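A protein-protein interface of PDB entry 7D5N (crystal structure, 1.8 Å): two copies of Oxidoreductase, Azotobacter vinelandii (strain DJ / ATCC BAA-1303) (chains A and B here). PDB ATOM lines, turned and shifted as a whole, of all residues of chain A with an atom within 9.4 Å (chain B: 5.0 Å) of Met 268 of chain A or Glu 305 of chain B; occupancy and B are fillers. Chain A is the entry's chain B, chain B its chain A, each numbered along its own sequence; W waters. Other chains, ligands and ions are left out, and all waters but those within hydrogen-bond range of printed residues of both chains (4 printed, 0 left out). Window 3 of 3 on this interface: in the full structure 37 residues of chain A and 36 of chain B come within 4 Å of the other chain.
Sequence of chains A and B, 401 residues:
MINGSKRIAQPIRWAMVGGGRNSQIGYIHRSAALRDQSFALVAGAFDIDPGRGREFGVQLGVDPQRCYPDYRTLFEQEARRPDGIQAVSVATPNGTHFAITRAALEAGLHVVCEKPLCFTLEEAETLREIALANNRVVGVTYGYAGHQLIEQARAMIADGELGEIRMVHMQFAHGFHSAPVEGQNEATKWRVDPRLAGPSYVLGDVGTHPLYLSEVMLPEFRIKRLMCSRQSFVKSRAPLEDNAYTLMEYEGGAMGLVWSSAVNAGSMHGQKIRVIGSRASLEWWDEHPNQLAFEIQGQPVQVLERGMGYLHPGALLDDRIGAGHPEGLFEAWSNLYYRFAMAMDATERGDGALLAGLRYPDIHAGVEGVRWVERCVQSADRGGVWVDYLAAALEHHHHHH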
ATOM      1  N   TYR A 144     -39.323 -17.071   4.655  1.00  0.00           N
ATOM      2  CA  TYR A 144     -38.811 -17.462   5.992  1.00  0.00           C
ATOM      3  C   TYR A 144     -39.829 -18.387   6.666  1.00  0.00           C
ATOM      4  O   TYR A 144     -39.440 -19.181   7.538  1.00  0.00           O
ATOM      5  CB  TYR A 144     -38.480 -16.217   6.813  1.00  0.00           C
ATOM      6  CG  TYR A 144     -37.487 -15.311   6.134  1.00  0.00           C
ATOM      7  CD1 TYR A 144     -36.123 -15.574   6.156  1.00  0.00           C
ATOM      8  CD2 TYR A 144     -37.919 -14.190   5.450  1.00  0.00           C
ATOM      9  CE1 TYR A 144     -35.217 -14.754   5.504  1.00  0.00           C
ATOM     10  CE2 TYR A 144     -37.030 -13.369   4.778  1.00  0.00           C
ATOM     11  CZ  TYR A 144     -35.672 -13.648   4.813  1.00  0.00           C
ATOM     12  OH  TYR A 144     -34.792 -12.828   4.175  1.00  0.00           O
ATOM     13  N   GLN A 171     -38.356  -7.873  14.611  1.00  0.00           N
ATOM     14  CA  GLN A 171     -37.530  -6.894  13.881  1.00  0.00           C
ATOM     15  C   GLN A 171     -37.099  -7.531  12.581  1.00  0.00           C
ATOM     16  O   GLN A 171     -36.957  -8.765  12.515  1.00  0.00           O
ATOM     17  CB  GLN A 171     -36.326  -6.433  14.703  1.00  0.00           C
ATOM     18  CG  GLN A 171     -35.400  -7.569  15.124  1.00  0.00           C
ATOM     19  CD  GLN A 171     -34.152  -7.046  15.789  1.00  0.00           C
ATOM     20  OE1 GLN A 171     -34.188  -6.601  16.924  1.00  0.00           O
ATOM     21  NE2 GLN A 171     -33.034  -7.093  15.088  1.00  0.00           N
ATOM     22  N   PHE A 172     -36.852  -6.676  11.613  1.00  0.00           N
ATOM     23  CA  PHE A 172     -35.979  -6.993  10.470  1.00  0.00           C
ATOM     24  C   PHE A 172     -35.183  -5.728  10.249  1.00  0.00           C
ATOM     25  O   PHE A 172     -35.694  -4.767   9.683  1.00  0.00           O
ATOM     26  CB  PHE A 172     -36.816  -7.441   9.282  1.00  0.00           C
ATOM     27  CG  PHE A 172     -36.053  -8.142   8.192  1.00  0.00           C
ATOM     28  CD1 PHE A 172     -36.711  -9.023   7.361  1.00  0.00           C
ATOM     29  CD2 PHE A 172     -34.688  -7.951   8.010  1.00  0.00           C
ATOM     30  CE1 PHE A 172     -36.039  -9.672   6.340  1.00  0.00           C
ATOM     31  CE2 PHE A 172     -34.007  -8.625   7.003  1.00  0.00           C
ATOM     32  CZ  PHE A 172     -34.692  -9.477   6.167  1.00  0.00           C
ATOM     33  N   ALA A 173     -33.980  -5.704  10.803  1.00  0.00           N
ATOM     34  CA  ALA A 173     -33.192  -4.465  10.915  1.00  0.00           C
ATOM     35  C   ALA A 173     -31.772  -4.757  10.444  1.00  0.00           C
ATOM     36  O   ALA A 173     -30.946  -5.232  11.255  1.00  0.00           O
ATOM     37  CB  ALA A 173     -33.239  -3.950  12.328  1.00  0.00           C
ATOM     38  N   HIS A 174     -31.514  -4.519   9.159  1.00  0.00           N
ATOM     39  CA  HIS A 174     -30.173  -4.725   8.554  1.00  0.00           C
ATOM     40  C   HIS A 174     -29.519  -3.362   8.338  1.00  0.00           C
ATOM     41  O   HIS A 174     -30.225  -2.340   8.474  1.00  0.00           O
ATOM     42  CB  HIS A 174     -30.261  -5.568   7.276  1.00  0.00           C
ATOM     43  CG  HIS A 174     -30.957  -4.896   6.148  1.00  0.00           C
ATOM     44  ND1 HIS A 174     -30.320  -3.945   5.348  1.00  0.00           N
ATOM     45  CD2 HIS A 174     -32.223  -5.019   5.683  1.00  0.00           C
ATOM     46  CE1 HIS A 174     -31.174  -3.522   4.436  1.00  0.00           C
ATOM     47  NE2 HIS A 174     -32.350  -4.164   4.626  1.00  0.00           N
ATOM     48  N   GLY A 175     -28.226  -3.356   8.017  1.00  0.00           N
ATOM     49  CA  GLY A 175     -27.456  -2.113   7.854  1.00  0.00           C
ATOM     50  C   GLY A 175     -27.054  -1.824   6.416  1.00  0.00           C
ATOM     51  O   GLY A 175     -26.349  -0.833   6.206  1.00  0.00           O
ATOM     52  N   PHE A 176     -27.493  -2.608   5.442  1.00  0.00           N
ATOM     53  CA  PHE A 176     -26.952  -2.504   4.058  1.00  0.00           C
ATOM     54  C   PHE A 176     -27.203  -1.124   3.456  1.00  0.00           C
ATOM     55  O   PHE A 176     -26.393  -0.734   2.594  1.00  0.00           O
ATOM     56  CB  PHE A 176     -27.438  -3.640   3.161  1.00  0.00           C
ATOM     57  CG  PHE A 176     -26.830  -4.969   3.510  1.00  0.00           C
ATOM     58  CD1 PHE A 176     -25.503  -5.251   3.225  1.00  0.00           C
ATOM     59  CD2 PHE A 176     -27.604  -5.956   4.097  1.00  0.00           C
ATOM     60  CE1 PHE A 176     -24.959  -6.486   3.552  1.00  0.00           C
ATOM     61  CE2 PHE A 176     -27.063  -7.187   4.407  1.00  0.00           C
ATOM     62  CZ  PHE A 176     -25.744  -7.447   4.142  1.00  0.00           C
ATOM     63  N   HIS A 177     -28.216  -0.379   3.905  1.00  0.00           N
ATOM     64  CA  HIS A 177     -28.500   0.950   3.313  1.00  0.00           C
ATOM     65  C   HIS A 177     -28.225   2.080   4.303  1.00  0.00           C
ATOM     66  O   HIS A 177     -28.786   3.159   4.103  1.00  0.00           O
ATOM     67  CB  HIS A 177     -29.886   0.978   2.663  1.00  0.00           C
ATOM     68  CG  HIS A 177     -30.064  -0.114   1.666  1.00  0.00           C
ATOM     69  ND1 HIS A 177     -31.280  -0.737   1.471  1.00  0.00           N
ATOM     70  CD2 HIS A 177     -29.188  -0.709   0.825  1.00  0.00           C
ATOM     71  CE1 HIS A 177     -31.139  -1.677   0.555  1.00  0.00           C
ATOM     72  NE2 HIS A 177     -29.871  -1.672   0.133  1.00  0.00           N
ATOM     73  N   SER A 178     -27.327   1.884   5.265  1.00  0.00           N
ATOM     74  CA  SER A 178     -26.862   2.962   6.172  1.00  0.00           C
ATOM     75  C   SER A 178     -26.274   4.118   5.355  1.00  0.00           C
ATOM     76  O   SER A 178     -26.483   5.294   5.725  1.00  0.00           O
ATOM     77  CB  SER A 178     -25.853   2.454   7.151  1.00  0.00           C
ATOM     78  OG  SER A 178     -26.382   1.362   7.883  1.00  0.00           O
ATOM     79  N   SER A 261     -35.856  -1.817   9.610  1.00  0.00           N
ATOM     80  CA  SER A 261     -34.714  -0.913   9.350  1.00  0.00           C
ATOM     81  C   SER A 261     -33.824  -1.429   8.228  1.00  0.00           C
ATOM     82  O   SER A 261     -33.589  -2.650   8.118  1.00  0.00           O
ATOM     83  CB  SER A 261     -33.931  -0.681  10.609  1.00  0.00           C
ATOM     84  OG  SER A 261     -32.974   0.357  10.433  1.00  0.00           O
ATOM     85  N   ASN A 264     -29.574  -0.127  10.195  1.00  0.00           N
ATOM     86  CA  ASN A 264     -29.007  -0.704  11.438  1.00  0.00           C
ATOM     87  C   ASN A 264     -27.548  -1.081  11.158  1.00  0.00           C
ATOM     88  O   ASN A 264     -27.272  -2.269  10.930  1.00  0.00           O
ATOM     89  CB  ASN A 264     -29.833  -1.902  11.908  1.00  0.00           C
ATOM     90  CG  ASN A 264     -29.326  -2.458  13.214  1.00  0.00           C
ATOM     91  OD1 ASN A 264     -28.549  -1.793  13.908  1.00  0.00           O
ATOM     92  ND2 ASN A 264     -29.742  -3.678  13.540  1.00  0.00           N
ATOM     93  N   ALA A 265     -26.661  -0.088  11.135  1.00  0.00           N
ATOM     94  CA  ALA A 265     -25.266  -0.230  10.652  1.00  0.00           C
ATOM     95  C   ALA A 265     -24.583  -1.423  11.337  1.00  0.00           C
ATOM     96  O   ALA A 265     -24.657  -1.532  12.589  1.00  0.00           O
ATOM     97  CB  ALA A 265     -24.512   1.045  10.918  1.00  0.00           C
ATOM     98  N   GLY A 266     -23.973  -2.309  10.552  1.00  0.00           N
ATOM     99  CA  GLY A 266     -23.254  -3.485  11.082  1.00  0.00           C
ATOM    100  C   GLY A 266     -24.113  -4.744  11.129  1.00  0.00           C
ATOM    101  O   GLY A 266     -23.567  -5.859  11.269  1.00  0.00           O
ATOM    102  N   SER A 267     -25.429  -4.620  10.999  1.00  0.00           N
ATOM    103  CA  SER A 267     -26.328  -5.793  11.103  1.00  0.00           C
ATOM    104  C   SER A 267     -26.390  -6.489   9.746  1.00  0.00           C
ATOM    105  O   SER A 267     -26.719  -5.834   8.733  1.00  0.00           O
ATOM    106  CB  SER A 267     -27.698  -5.428  11.599  1.00  0.00           C
ATOM    107  OG  SER A 267     -28.610  -6.501  11.354  1.00  0.00           O
ATOM    108  N   MET A 268     -26.140  -7.796   9.745  1.00  0.00           N
ATOM    109  CA  MET A 268     -26.062  -8.590   8.504  1.00  0.00           C
ATOM    110  C   MET A 268     -27.461  -8.924   7.990  1.00  0.00           C
ATOM    111  O   MET A 268     -27.561  -9.239   6.809  1.00  0.00           O
ATOM    112  CB  MET A 268     -25.246  -9.864   8.743  1.00  0.00           C
ATOM    113  CG  MET A 268     -23.764  -9.569   8.918  1.00  0.00           C
ATOM    114  SD  MET A 268     -23.046  -8.934   7.358  1.00  0.00           S
ATOM    115  CE  MET A 268     -23.729 -10.101   6.191  1.00  0.00           C
ATOM    116  N   HIS A 269     -28.496  -8.862   8.840  1.00  0.00           N
ATOM    117  CA  HIS A 269     -29.889  -9.215   8.465  1.00  0.00           C
ATOM    118  C   HIS A 269     -30.806  -8.880   9.641  1.00  0.00           C
ATOM    119  O   HIS A 269     -31.668  -8.002   9.491  1.00  0.00           O
ATOM    120  CB  HIS A 269     -29.996 -10.687   8.037  1.00  0.00           C
ATOM    121  CG  HIS A 269     -30.604 -10.842   6.685  1.00  0.00           C
ATOM    122  ND1 HIS A 269     -31.699 -11.665   6.450  1.00  0.00           N
ATOM    123  CD2 HIS A 269     -30.287 -10.274   5.502  1.00  0.00           C
ATOM    124  CE1 HIS A 269     -32.005 -11.617   5.168  1.00  0.00           C
ATOM    125  NE2 HIS A 269     -31.173 -10.747   4.565  1.00  0.00           N
ATOM    126  N   GLY A 270     -30.567  -9.511  10.789  1.00  0.00           N
ATOM    127  CA  GLY A 270     -31.242  -9.128  12.043  1.00  0.00           C
ATOM    128  C   GLY A 270     -32.748  -9.291  11.953  1.00  0.00           C
ATOM    129  O   GLY A 270     -33.473  -8.404  12.459  1.00  0.00           O
ATOM    130  N   GLN A 271     -33.228 -10.369  11.334  1.00  0.00           N
ATOM    131  CA  GLN A 271     -34.675 -10.668  11.387  1.00  0.00           C
ATOM    132  C   GLN A 271     -34.891 -11.558  12.606  1.00  0.00           C
ATOM    133  O   GLN A 271     -34.324 -12.654  12.643  1.00  0.00           O
ATOM    134  CB  GLN A 271     -35.205 -11.324  10.119  1.00  0.00           C
ATOM    135  CG  GLN A 271     -36.690 -11.569  10.206  1.00  0.00           C
ATOM    136  CD  GLN A 271     -37.319 -12.259   9.026  1.00  0.00           C
ATOM    137  OE1 GLN A 271     -38.534 -12.391   8.963  1.00  0.00           O
ATOM    138  NE2 GLN A 271     -36.506 -12.740   8.102  1.00  0.00           N
ATOM    139  N   LYS A 272     -35.641 -11.083  13.588  1.00  0.00           N
ATOM    140  CA  LYS A 272     -35.874 -11.870  14.819  1.00  0.00           C
ATOM    141  C   LYS A 272     -37.330 -11.742  15.241  1.00  0.00           C
ATOM    142  O   LYS A 272     -37.942 -10.687  14.998  1.00  0.00           O
ATOM    143  CB  LYS A 272     -34.956 -11.445  15.961  1.00  0.00           C
ATOM    144  CG  LYS A 272     -33.468 -11.502  15.644  1.00  0.00           C
ATOM    145  CD  LYS A 272     -32.558 -10.875  16.688  1.00  0.00           C
ATOM    146  CE  LYS A 272     -31.100 -10.945  16.266  1.00  0.00           C
ATOM    147  NZ  LYS A 272     -30.173 -10.790  17.408  1.00  0.00           N
ATOM    148  N   TRP A 285     -34.254 -16.473  14.950  1.00  0.00           N
ATOM    149  CA  TRP A 285     -33.375 -15.508  14.261  1.00  0.00           C
ATOM    150  C   TRP A 285     -33.029 -16.064  12.877  1.00  0.00           C
ATOM    151  O   TRP A 285     -32.487 -17.187  12.813  1.00  0.00           O
ATOM    152  CB  TRP A 285     -32.160 -15.273  15.151  1.00  0.00           C
ATOM    153  CG  TRP A 285     -31.103 -14.427  14.535  1.00  0.00           C
ATOM    154  CD1 TRP A 285     -31.230 -13.539  13.506  1.00  0.00           C
ATOM    155  CD2 TRP A 285     -29.743 -14.339  14.982  1.00  0.00           C
ATOM    156  NE1 TRP A 285     -30.026 -12.936  13.254  1.00  0.00           N
ATOM    157  CE2 TRP A 285     -29.100 -13.398  14.148  1.00  0.00           C
ATOM    158  CE3 TRP A 285     -29.019 -14.963  15.999  1.00  0.00           C
ATOM    159  CZ2 TRP A 285     -27.748 -13.086  14.297  1.00  0.00           C
ATOM    160  CZ3 TRP A 285     -27.687 -14.646  16.151  1.00  0.00           C
ATOM    161  CH2 TRP A 285     -27.064 -13.722  15.304  1.00  0.00           C
ATOM    162  N   ASP A 286     -33.348 -15.315  11.815  1.00  0.00           N
ATOM    163  CA  ASP A 286     -33.312 -15.830  10.423  1.00  0.00           C
ATOM    164  C   ASP A 286     -31.902 -16.296  10.051  1.00  0.00           C
ATOM    165  O   ASP A 286     -31.808 -17.184   9.197  1.00  0.00           O
ATOM    166  CB  ASP A 286     -33.858 -14.830   9.395  1.00  0.00           C
ATOM    167  CG  ASP A 286     -33.049 -13.568   9.124  1.00  0.00           C
ATOM    168  OD1 ASP A 286     -32.259 -13.158  10.005  1.00  0.00           O
ATOM    169  OD2 ASP A 286     -33.253 -12.985   8.015  1.00  0.00           O
ATOM    170  N   GLU A 287     -30.848 -15.703  10.619  1.00  0.00           N
ATOM    171  CA  GLU A 287     -29.464 -16.017  10.186  1.00  0.00           C
ATOM    172  C   GLU A 287     -29.031 -17.368  10.770  1.00  0.00           C
ATOM    173  O   GLU A 287     -28.071 -17.967  10.247  1.00  0.00           O
ATOM    174  CB  GLU A 287     -28.492 -14.921  10.609  1.00  0.00           C
ATOM    175  CG  GLU A 287     -28.751 -13.581   9.938  1.00  0.00           C
ATOM    176  CD  GLU A 287     -27.943 -12.434  10.529  1.00  0.00           C
ATOM    177  OE1 GLU A 287     -26.720 -12.471  10.365  1.00  0.00           O
ATOM    178  OE2 GLU A 287     -28.547 -11.498  11.137  1.00  0.00           O
ATOM    179  N   HIS A 288     -29.728 -17.836  11.810  1.00  0.00           N
ATOM    180  CA  HIS A 288     -29.487 -19.147  12.452  1.00  0.00           C
ATOM    181  C   HIS A 288     -30.821 -19.862  12.515  1.00  0.00           C
ATOM    182  O   HIS A 288     -31.350 -20.071  13.599  1.00  0.00           O
ATOM    183  CB  HIS A 288     -28.782 -18.976  13.803  1.00  0.00           C
ATOM    184  CG  HIS A 288     -27.467 -18.303  13.633  1.00  0.00           C
ATOM    185  ND1 HIS A 288     -26.408 -18.907  12.986  1.00  0.00           N
ATOM    186  CD2 HIS A 288     -27.052 -17.062  13.952  1.00  0.00           C
ATOM    187  CE1 HIS A 288     -25.385 -18.076  12.951  1.00  0.00           C
ATOM    188  NE2 HIS A 288     -25.756 -16.934  13.529  1.00  0.00           N
ATOM    189  N   LEU B 149     -16.628 -20.073   2.615  1.00  0.00           N
ATOM    190  CA  LEU B 149     -15.647 -19.532   3.586  1.00  0.00           C
ATOM    191  C   LEU B 149     -14.481 -20.505   3.788  1.00  0.00           C
ATOM    192  O   LEU B 149     -13.451 -20.077   4.329  1.00  0.00           O
ATOM    193  CB  LEU B 149     -16.350 -19.177   4.899  1.00  0.00           C
ATOM    194  CG  LEU B 149     -17.280 -17.974   4.797  1.00  0.00           C
ATOM    195  CD1 LEU B 149     -18.038 -17.772   6.088  1.00  0.00           C
ATOM    196  CD2 LEU B 149     -16.503 -16.710   4.421  1.00  0.00           C
ATOM    197  N   ASN B 290     -21.815 -20.052   7.475  1.00  0.00           N
ATOM    198  CA  ASN B 290     -21.784 -18.743   6.779  1.00  0.00           C
ATOM    199  C   ASN B 290     -20.911 -17.732   7.526  1.00  0.00           C
ATOM    200  O   ASN B 290     -20.853 -16.574   7.065  1.00  0.00           O
ATOM    201  CB  ASN B 290     -23.189 -18.197   6.574  1.00  0.00           C
ATOM    202  CG  ASN B 290     -24.035 -19.177   5.783  1.00  0.00           C
ATOM    203  OD1 ASN B 290     -23.609 -19.656   4.732  1.00  0.00           O
ATOM    204  ND2 ASN B 290     -25.172 -19.564   6.339  1.00  0.00           N
ATOM    205  N   GLN B 291     -20.269 -18.134   8.625  1.00  0.00           N
ATOM    206  CA  GLN B 291     -19.369 -17.245   9.388  1.00  0.00           C
ATOM    207  C   GLN B 291     -17.984 -17.885   9.519  1.00  0.00           C
ATOM    208  O   GLN B 291     -17.874 -19.119   9.586  1.00  0.00           O
ATOM    209  CB  GLN B 291     -19.936 -16.962  10.771  1.00  0.00           C
ATOM    210  CG  GLN B 291     -21.139 -16.028  10.748  1.00  0.00           C
ATOM    211  CD  GLN B 291     -22.450 -16.731  10.473  1.00  0.00           C
ATOM    212  OE1 GLN B 291     -22.726 -17.794  11.029  1.00  0.00           O
ATOM    213  NE2 GLN B 291     -23.257 -16.144   9.602  1.00  0.00           N
ATOM    214  N   VAL B 303     -15.631 -11.420  12.833  1.00  0.00           N
ATOM    215  CA  VAL B 303     -16.370 -12.498  12.138  1.00  0.00           C
ATOM    216  C   VAL B 303     -16.478 -12.093  10.682  1.00  0.00           C
ATOM    217  O   VAL B 303     -17.029 -11.036  10.391  1.00  0.00           O
ATOM    218  CB  VAL B 303     -17.743 -12.767  12.764  1.00  0.00           C
ATOM    219  CG1 VAL B 303     -18.449 -13.884  12.018  1.00  0.00           C
ATOM    220  CG2 VAL B 303     -17.631 -13.053  14.255  1.00  0.00           C
ATOM    221  N   LEU B 304     -15.994 -12.959   9.806  1.00  0.00           N
ATOM    222  CA  LEU B 304     -16.155 -12.780   8.346  1.00  0.00           C
ATOM    223  C   LEU B 304     -17.440 -13.485   7.917  1.00  0.00           C
ATOM    224  O   LEU B 304     -17.639 -14.651   8.316  1.00  0.00           O
ATOM    225  CB  LEU B 304     -14.952 -13.350   7.603  1.00  0.00           C
ATOM    226  CG  LEU B 304     -13.573 -12.912   8.074  1.00  0.00           C
ATOM    227  CD1 LEU B 304     -12.520 -13.444   7.118  1.00  0.00           C
ATOM    228  CD2 LEU B 304     -13.456 -11.404   8.163  1.00  0.00           C
ATOM    229  N   GLU B 305     -18.246 -12.809   7.110  1.00  0.00           N
ATOM    230  CA  GLU B 305     -19.564 -13.304   6.652  1.00  0.00           C
ATOM    231  C   GLU B 305     -19.510 -13.667   5.174  1.00  0.00           C
ATOM    232  O   GLU B 305     -18.948 -12.900   4.390  1.00  0.00           O
ATOM    233  CB  GLU B 305     -20.637 -12.241   6.873  1.00  0.00           C
ATOM    234  CG  GLU B 305     -21.070 -12.144   8.318  1.00  0.00           C
ATOM    235  CD  GLU B 305     -22.233 -13.028   8.725  1.00  0.00           C
ATOM    236  OE1 GLU B 305     -22.882 -13.638   7.835  1.00  0.00           O
ATOM    237  OE2 GLU B 305     -22.519 -13.064   9.946  1.00  0.00           O
ATOM    238  N   ARG B 306     -20.173 -14.756   4.823  1.00  0.00           N
ATOM    239  CA  ARG B 306     -20.412 -15.166   3.421  1.00  0.00           C
ATOM    240  C   ARG B 306     -20.995 -13.995   2.639  1.00  0.00           C
ATOM    241  O   ARG B 306     -21.909 -13.311   3.147  1.00  0.00           O
ATOM    242  CB  ARG B 306     -21.416 -16.320   3.366  1.00  0.00           C
ATOM    243  CG  ARG B 306     -21.593 -16.896   1.969  1.00  0.00           C
ATOM    244  CD  ARG B 306     -22.844 -17.743   1.895  1.00  0.00           C
ATOM    245  NE  ARG B 306     -24.038 -16.935   2.116  1.00  0.00           N
ATOM    246  CZ  ARG B 306     -24.601 -16.139   1.215  1.00  0.00           C
ATOM    247  NH1 ARG B 306     -24.080 -16.023   0.006  1.00  0.00           N
ATOM    248  NH2 ARG B 306     -25.708 -15.471   1.524  1.00  0.00           N
ATOM    249  N   GLY B 307     -20.498 -13.779   1.427  1.00  0.00           N
ATOM    250  CA  GLY B 307     -21.116 -12.865   0.461  1.00  0.00           C
ATOM    251  C   GLY B 307     -20.668 -11.426   0.637  1.00  0.00           C
ATOM    252  O   GLY B 307     -21.142 -10.576  -0.118  1.00  0.00           O
ATOM    253  N   MET B 308     -19.802 -11.118   1.597  1.00  0.00           N
ATOM    254  CA  MET B 308     -19.407  -9.709   1.826  1.00  0.00           C
ATOM    255  C   MET B 308     -18.243  -9.329   0.900  1.00  0.00           C
ATOM    256  O   MET B 308     -17.355 -10.193   0.627  1.00  0.00           O
ATOM    257  CB  MET B 308     -19.050  -9.474   3.290  1.00  0.00           C
ATOM    258  CG  MET B 308     -20.275  -9.523   4.195  1.00  0.00           C
ATOM    259  SD  MET B 308     -21.551  -8.277   3.793  1.00  0.00           S
ATOM    260  CE  MET B 308     -20.785  -6.838   4.538  1.00  0.00           C
ATOM    261  N   TYR B 310     -15.571  -7.682   1.324  1.00  0.00           N
ATOM    262  CA  TYR B 310     -14.195  -7.760   1.883  1.00  0.00           C
ATOM    263  C   TYR B 310     -13.566  -9.158   1.672  1.00  0.00           C
ATOM    264  O   TYR B 310     -12.353  -9.313   1.945  1.00  0.00           O
ATOM    265  CB  TYR B 310     -14.167  -7.341   3.353  1.00  0.00           C
ATOM    266  CG  TYR B 310     -15.158  -8.053   4.254  1.00  0.00           C
ATOM    267  CD1 TYR B 310     -15.031  -9.402   4.554  1.00  0.00           C
ATOM    268  CD2 TYR B 310     -16.203  -7.369   4.839  1.00  0.00           C
ATOM    269  CE1 TYR B 310     -15.938 -10.053   5.383  1.00  0.00           C
ATOM    270  CE2 TYR B 310     -17.093  -7.993   5.712  1.00  0.00           C
ATOM    271  CZ  TYR B 310     -16.971  -9.343   5.977  1.00  0.00           C
ATOM    272  OH  TYR B 310     -17.854  -9.979   6.815  1.00  0.00           O
ATOM    273  N   LEU B 311     -14.336 -10.152   1.216  1.00  0.00           N
ATOM    274  CA  LEU B 311     -13.816 -11.529   1.003  1.00  0.00           C
ATOM    275  C   LEU B 311     -12.907 -11.557  -0.232  1.00  0.00           C
ATOM    276  O   LEU B 311     -13.006 -10.655  -1.080  1.00  0.00           O
ATOM    277  CB  LEU B 311     -14.959 -12.522   0.826  1.00  0.00           C
ATOM    278  CG  LEU B 311     -15.877 -12.709   2.027  1.00  0.00           C
ATOM    279  CD1 LEU B 311     -16.988 -13.700   1.704  1.00  0.00           C
ATOM    280  CD2 LEU B 311     -15.100 -13.158   3.248  1.00  0.00           C
ATOM    281  N   ALA B 323     -25.529 -11.540   0.848  1.00  0.00           N
ATOM    282  CA  ALA B 323     -24.989 -11.721   2.211  1.00  0.00           C
ATOM    283  C   ALA B 323     -26.126 -11.554   3.232  1.00  0.00           C
ATOM    284  O   ALA B 323     -26.983 -10.705   3.032  1.00  0.00           O
ATOM    285  CB  ALA B 323     -23.893 -10.726   2.470  1.00  0.00           C
ATOM    286  N   GLY B 324     -26.125 -12.358   4.286  1.00  0.00           N
ATOM    287  CA  GLY B 324     -27.111 -12.209   5.371  1.00  0.00           C
ATOM    288  C   GLY B 324     -28.221 -13.232   5.265  1.00  0.00           C
ATOM    289  O   GLY B 324     -28.801 -13.594   6.319  1.00  0.00           O
HETATM  290  O   HOH W   1     -26.838 -20.362   9.241  1.00  0.00           O
HETATM  291  O   HOH W   2     -19.825  -8.504   7.982  1.00  0.00           O
HETATM  292  O   HOH W   3     -25.940 -17.182   8.708  1.00  0.00           O
HETATM  293  O   HOH W   4     -25.594 -13.540   8.149  1.00  0.00           O
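A ring nitrogen (ND1) of His 269 of chain A sits close to the backbone carbonyl oxygen of Gly 324 of chain B (3.5 Å).
The side-chain carboxylate of Glu 287 of chain A lies within hydrogen-bond range of the indole nitrogen of Trp 285 of chain A, at 3.0 Å. The side-chain carboxylate (OE2) of Glu 287 of chain A sits at hydrogen-bond distance from the backbone NH (N) of His 269 of chain A, at 3.5 Å. ND1 of His 269 of chain A lies within hydrogen-bond range of OD2 of Asp 286 of chain A (2.6 Å). N of Gly 270 of chain A lies within hydrogen-bond range of OE2 of Glu 287 of chain A (2.9 Å). ND1 of His 174 of chain A is in hydrogen-bond range of N of Phe 176 of chain A (3.1 Å). The backbone NH (N) of Glu 305 of chain B is in hydrogen-bond range of the side-chain hydroxyl (OH) of Tyr 310 of chain B (2.9 Å).
Among the printed residues, merely in contact across the chains: Phe 176 of chain A with Met 308 of chain B (3.9 Å), Phe 176 of chain A with Ala 323 of chain B (3.7 Å), Met 268 of chain A with Glu 305 of chain B (3.8 Å), Met 268 of chain A with Met 308 of chain B (3.7 Å), Met 268 of chain A with Ala 323 of chain B (3.8 Å), Met 268 of chain A with Gly 324 of chain B (3.3 Å), Glu 287 of chain A with Gly 324 of chain B (3.6 Å) and His 288 of chain A with Gln 291 of chain B (3.3 Å).
Gly 175 of chain A touches none of the printed residues of chain B. Gly 266 of chain A touches none of the printed residues of chain B. Of chain B, only Glu 305, Met 308, Ala 323 and Gly 324 come within 4 Å of Met 268 of chain A. Of the printed residues of chain B, His 269 of chain A touches Gly 324 (3.3 Å). Printed residues of chain B within 4 Å of His 288 of chain A: Gln 291 (3.3 Å). Glu 305 of chain B touches just one residue of chain A: Met 268 (3.8 Å). Printed residues of chain A within 4 Å of Met 308 of chain B: Phe 176 (3.9 Å) and Met 268 (3.7 Å). Gly 324 of chain B touches just these residues of chain A: Met 268 (3.3 Å), His 269 (3.3 Å) and Glu 287 (3.6 Å). The nearest residue of chain B that does not touch Met 268 of chain A is Arg 306 of chain B (4.8 Å).
Of the 13 printed residues of chain B, 5 touch a printed residue of chain A. Hydrophobic or aromatic side chains of chain B that line the printed part of chain A: Met 308 and Ala 323.
No position is printed for both chains.
Water W4 lies within hydrogen-bond range of OE1 of Glu 287 of chain A and OE1 of Glu 305 of chain B. Water W2 lies within hydrogen-bond range of OH of Tyr 310 of chain B (2.7 Å) and SD of Met 268 of chain A (3.3 Å). Water W3 lies within hydrogen-bond range of the backbone carbonyl oxygen (O) of Glu 287 of chain A (2.7 Å), the side-chain amide nitrogen (NE2) of Gln 291 of chain B (3.0 Å) and the side-chain amide nitrogen (ND2) of Asn 290 of chain B (3.4 Å). Water W1 lies within hydrogen-bond range of the backbone carbonyl oxygen of Glu 287 of chain A (2.9 Å) and the side-chain amide nitrogen of Asn 290 of chain B (3.4 Å).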
